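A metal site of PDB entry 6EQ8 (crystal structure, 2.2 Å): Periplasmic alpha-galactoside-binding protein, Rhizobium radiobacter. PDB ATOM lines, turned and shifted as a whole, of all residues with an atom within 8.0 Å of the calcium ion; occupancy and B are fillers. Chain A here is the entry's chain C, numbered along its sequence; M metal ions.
OD1 of Asp 185 sits at hydrogen-bond distance from N of Asn 187, at 3.1 Å. O of Tyr 178 lies within hydrogen-bond range of N of Val 183, 3.0 Å away. The backbone NH of Asp 185 sits at hydrogen-bond distance from the backbone carbonyl oxygen of Glu 180, at 3.1 Å.
The calcium ion is bound by O of Asp 185 (2.4 Å), O of Val 188 (2.5 Å), O of Ala 182 (2.5 Å) and O of Val 183 (2.6 Å). The calcium ion has four donor atoms within binding distance.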
ATOM      1  N   ILE A 103      15.232   8.438   9.882  1.00  0.00           N
ATOM      2  CA  ILE A 103      15.172   8.838   8.467  1.00  0.00           C
ATOM      3  C   ILE A 103      14.781   7.640   7.529  1.00  0.00           C
ATOM      4  O   ILE A 103      14.354   7.872   6.406  1.00  0.00           O
ATOM      5  CB  ILE A 103      16.447   9.598   8.012  1.00  0.00           C
ATOM      6  CG1 ILE A 103      17.687   8.675   7.901  1.00  0.00           C
ATOM      7  CG2 ILE A 103      16.708  10.806   8.932  1.00  0.00           C
ATOM      8  CD1 ILE A 103      18.699   9.149   6.960  1.00  0.00           C
ATOM      9  N   TYR A 178      20.040  13.488   3.840  1.00  0.00           N
ATOM     10  CA  TYR A 178      18.633  13.308   4.141  1.00  0.00           C
ATOM     11  C   TYR A 178      17.756  13.551   2.894  1.00  0.00           C
ATOM     12  O   TYR A 178      16.902  12.725   2.592  1.00  0.00           O
ATOM     13  CB  TYR A 178      18.193  14.179   5.335  1.00  0.00           C
ATOM     14  CG  TYR A 178      16.715  14.029   5.611  1.00  0.00           C
ATOM     15  CD1 TYR A 178      16.206  12.854   6.142  1.00  0.00           C
ATOM     16  CD2 TYR A 178      15.808  15.023   5.241  1.00  0.00           C
ATOM     17  CE1 TYR A 178      14.830  12.676   6.335  1.00  0.00           C
ATOM     18  CE2 TYR A 178      14.441  14.871   5.446  1.00  0.00           C
ATOM     19  CZ  TYR A 178      13.952  13.687   5.981  1.00  0.00           C
ATOM     20  OH  TYR A 178      12.606  13.516   6.162  1.00  0.00           O
ATOM     21  N   TRP A 179      18.010  14.648   2.161  1.00  0.00           N
ATOM     22  CA  TRP A 179      17.268  15.013   0.967  1.00  0.00           C
ATOM     23  C   TRP A 179      17.392  13.993  -0.167  1.00  0.00           C
ATOM     24  O   TRP A 179      16.388  13.469  -0.644  1.00  0.00           O
ATOM     25  CB  TRP A 179      17.657  16.426   0.479  1.00  0.00           C
ATOM     26  CG  TRP A 179      16.934  16.830  -0.783  1.00  0.00           C
ATOM     27  CD1 TRP A 179      17.464  16.939  -2.035  1.00  0.00           C
ATOM     28  CD2 TRP A 179      15.524  17.080  -0.919  1.00  0.00           C
ATOM     29  NE1 TRP A 179      16.480  17.281  -2.937  1.00  0.00           N
ATOM     30  CE2 TRP A 179      15.277  17.387  -2.281  1.00  0.00           C
ATOM     31  CE3 TRP A 179      14.442  17.106  -0.013  1.00  0.00           C
ATOM     32  CZ2 TRP A 179      13.999  17.688  -2.766  1.00  0.00           C
ATOM     33  CZ3 TRP A 179      13.173  17.430  -0.497  1.00  0.00           C
ATOM     34  CH2 TRP A 179      12.958  17.693  -1.862  1.00  0.00           C
ATOM     35  N   GLU A 180      18.620  13.714  -0.583  1.00  0.00           N
ATOM     36  CA  GLU A 180      18.910  12.791  -1.675  1.00  0.00           C
ATOM     37  C   GLU A 180      18.645  11.323  -1.366  1.00  0.00           C
ATOM     38  O   GLU A 180      18.023  10.616  -2.181  1.00  0.00           O
ATOM     39  CB  GLU A 180      20.360  12.952  -2.139  1.00  0.00           C
ATOM     40  CG  GLU A 180      20.647  14.233  -2.900  1.00  0.00           C
ATOM     41  CD  GLU A 180      22.115  14.582  -3.050  1.00  0.00           C
ATOM     42  OE1 GLU A 180      22.979  13.705  -2.791  1.00  0.00           O
ATOM     43  OE2 GLU A 180      22.413  15.738  -3.418  1.00  0.00           O
ATOM     44  N   ASP A 181      19.132  10.851  -0.202  1.00  0.00           N
ATOM     45  CA  ASP A 181      19.107   9.428   0.063  1.00  0.00           C
ATOM     46  C   ASP A 181      18.014   8.960   1.000  1.00  0.00           C
ATOM     47  O   ASP A 181      17.861   7.745   1.149  1.00  0.00           O
ATOM     48  CB  ASP A 181      20.501   8.972   0.527  1.00  0.00           C
ATOM     49  CG  ASP A 181      21.554   9.231  -0.556  1.00  0.00           C
ATOM     50  OD1 ASP A 181      21.222   9.100  -1.738  1.00  0.00           O
ATOM     51  OD2 ASP A 181      22.663   9.664  -0.211  1.00  0.00           O
ATOM     52  N   ALA A 182      17.161   9.859   1.507  1.00  0.00           N
ATOM     53  CA  ALA A 182      16.018   9.442   2.305  1.00  0.00           C
ATOM     54  C   ALA A 182      14.705   9.910   1.699  1.00  0.00           C
ATOM     55  O   ALA A 182      13.777   9.120   1.607  1.00  0.00           O
ATOM     56  CB  ALA A 182      16.152   9.912   3.768  1.00  0.00           C
ATOM     57  N   VAL A 183      14.617  11.203   1.278  1.00  0.00           N
ATOM     58  CA  VAL A 183      13.417  11.831   0.688  1.00  0.00           C
ATOM     59  C   VAL A 183      13.298  11.480  -0.800  1.00  0.00           C
ATOM     60  O   VAL A 183      12.274  10.925  -1.191  1.00  0.00           O
ATOM     61  CB  VAL A 183      13.362  13.377   0.909  1.00  0.00           C
ATOM     62  CG1 VAL A 183      12.153  13.997   0.216  1.00  0.00           C
ATOM     63  CG2 VAL A 183      13.361  13.723   2.396  1.00  0.00           C
ATOM     64  N   VAL A 184      14.303  11.852  -1.616  1.00  0.00           N
ATOM     65  CA  VAL A 184      14.339  11.621  -3.060  1.00  0.00           C
ATOM     66  C   VAL A 184      14.423  10.119  -3.363  1.00  0.00           C
ATOM     67  O   VAL A 184      13.742   9.658  -4.286  1.00  0.00           O
ATOM     68  CB  VAL A 184      15.433  12.468  -3.770  1.00  0.00           C
ATOM     69  CG1 VAL A 184      15.565  12.105  -5.257  1.00  0.00           C
ATOM     70  CG2 VAL A 184      15.141  13.960  -3.609  1.00  0.00           C
ATOM     71  N   ASP A 185      15.197   9.333  -2.562  1.00  0.00           N
ATOM     72  CA  ASP A 185      15.287   7.883  -2.734  1.00  0.00           C
ATOM     73  C   ASP A 185      13.880   7.242  -2.565  1.00  0.00           C
ATOM     74  O   ASP A 185      13.302   7.373  -1.493  1.00  0.00           O
ATOM     75  CB  ASP A 185      16.291   7.295  -1.747  1.00  0.00           C
ATOM     76  CG  ASP A 185      16.713   5.876  -2.061  1.00  0.00           C
ATOM     77  OD1 ASP A 185      15.829   5.045  -2.373  1.00  0.00           O
ATOM     78  OD2 ASP A 185      17.914   5.581  -1.967  1.00  0.00           O
ATOM     79  N   PRO A 186      13.288   6.598  -3.607  1.00  0.00           N
ATOM     80  CA  PRO A 186      11.906   6.078  -3.463  1.00  0.00           C
ATOM     81  C   PRO A 186      11.745   4.860  -2.551  1.00  0.00           C
ATOM     82  O   PRO A 186      10.621   4.560  -2.142  1.00  0.00           O
ATOM     83  CB  PRO A 186      11.495   5.765  -4.909  1.00  0.00           C
ATOM     84  CG  PRO A 186      12.796   5.474  -5.608  1.00  0.00           C
ATOM     85  CD  PRO A 186      13.823   6.371  -4.975  1.00  0.00           C
ATOM     86  N   ASN A 187      12.850   4.180  -2.223  1.00  0.00           N
ATOM     87  CA  ASN A 187      12.899   2.979  -1.398  1.00  0.00           C
ATOM     88  C   ASN A 187      13.011   3.247   0.100  1.00  0.00           C
ATOM     89  O   ASN A 187      13.010   2.306   0.908  1.00  0.00           O
ATOM     90  CB  ASN A 187      14.061   2.095  -1.869  1.00  0.00           C
ATOM     91  CG  ASN A 187      13.916   1.629  -3.292  1.00  0.00           C
ATOM     92  OD1 ASN A 187      13.011   0.859  -3.638  1.00  0.00           O
ATOM     93  ND2 ASN A 187      14.798   2.104  -4.162  1.00  0.00           N
ATOM     94  N   VAL A 188      13.125   4.535   0.470  1.00  0.00           N
ATOM     95  CA  VAL A 188      13.240   5.013   1.844  1.00  0.00           C
ATOM     96  C   VAL A 188      12.012   5.840   2.175  1.00  0.00           C
ATOM     97  O   VAL A 188      11.578   6.642   1.355  1.00  0.00           O
ATOM     98  CB  VAL A 188      14.566   5.803   2.119  1.00  0.00           C
ATOM     99  CG1 VAL A 188      14.758   6.080   3.605  1.00  0.00           C
ATOM    100  CG2 VAL A 188      15.783   5.081   1.564  1.00  0.00           C
ATOM    101  N   SER A 189      11.457   5.625   3.350  1.00  0.00           N
ATOM    102  CA  SER A 189      10.319   6.391   3.847  1.00  0.00           C
ATOM    103  C   SER A 189      10.623   6.906   5.243  1.00  0.00           C
ATOM    104  O   SER A 189      10.463   6.139   6.183  1.00  0.00           O
ATOM    105  CB  SER A 189       9.021   5.574   3.830  1.00  0.00           C
ATOM    106  OG  SER A 189       8.347   5.753   2.592  1.00  0.00           O
ATOM    107  N   PRO A 190      11.039   8.183   5.421  1.00  0.00           N
ATOM    108  CA  PRO A 190      11.272   8.710   6.800  1.00  0.00           C
ATOM    109  C   PRO A 190      10.024   8.644   7.705  1.00  0.00           C
ATOM    110  O   PRO A 190       8.890   8.601   7.208  1.00  0.00           O
ATOM    111  CB  PRO A 190      11.748  10.137   6.557  1.00  0.00           C
ATOM    112  CG  PRO A 190      12.254  10.149   5.116  1.00  0.00           C
ATOM    113  CD  PRO A 190      11.309   9.213   4.403  1.00  0.00           C
ATOM    114  N   ALA A 195       7.241  12.329   4.203  1.00  0.00           N
ATOM    115  CA  ALA A 195       8.476  12.892   3.662  1.00  0.00           C
ATOM    116  C   ALA A 195       8.792  12.412   2.215  1.00  0.00           C
ATOM    117  O   ALA A 195       9.830  11.815   1.939  1.00  0.00           O
ATOM    118  CB  ALA A 195       9.645  12.662   4.611  1.00  0.00           C
ATOM    119  N   SER A 196       7.879  12.718   1.297  1.00  0.00           N
ATOM    120  CA  SER A 196       8.007  12.435  -0.125  1.00  0.00           C
ATOM    121  C   SER A 196       8.573  13.706  -0.799  1.00  0.00           C
ATOM    122  O   SER A 196       8.433  14.780  -0.213  1.00  0.00           O
ATOM    123  CB  SER A 196       6.659  12.033  -0.724  1.00  0.00           C
ATOM    124  OG  SER A 196       5.675  13.054  -0.634  1.00  0.00           O
ATOM    125  N   PRO A 197       9.230  13.639  -1.990  1.00  0.00           N
ATOM    126  CA  PRO A 197       9.757  14.881  -2.601  1.00  0.00           C
ATOM    127  C   PRO A 197       8.707  15.952  -2.951  1.00  0.00           C
ATOM    128  O   PRO A 197       9.008  17.136  -2.837  1.00  0.00           O
ATOM    129  CB  PRO A 197      10.502  14.396  -3.852  1.00  0.00           C
ATOM    130  CG  PRO A 197      10.650  12.918  -3.689  1.00  0.00           C
ATOM    131  CD  PRO A 197       9.518  12.455  -2.819  1.00  0.00           C
ATOM    132  N   ARG A 554       2.236  10.719  -3.177  1.00  0.00           N
ATOM    133  CA  ARG A 554       2.265  10.130  -1.829  1.00  0.00           C
ATOM    134  C   ARG A 554       1.871  11.111  -0.687  1.00  0.00           C
ATOM    135  O   ARG A 554       1.994  10.732   0.474  1.00  0.00           O
ATOM    136  CB  ARG A 554       3.639   9.468  -1.533  1.00  0.00           C
ATOM    137  CG  ARG A 554       4.161   8.514  -2.617  1.00  0.00           C
ATOM    138  CD  ARG A 554       5.050   7.413  -2.055  1.00  0.00           C
ATOM    139  NE  ARG A 554       4.244   6.372  -1.402  1.00  0.00           N
ATOM    140  CZ  ARG A 554       4.281   6.072  -0.113  1.00  0.00           C
ATOM    141  NH1 ARG A 554       3.463   5.148   0.376  1.00  0.00           N
ATOM    142  NH2 ARG A 554       5.107   6.705   0.714  1.00  0.00           N
HETATM  143 CA    CA M   1      11.933   8.650  -0.053  1.00  0.00          CA
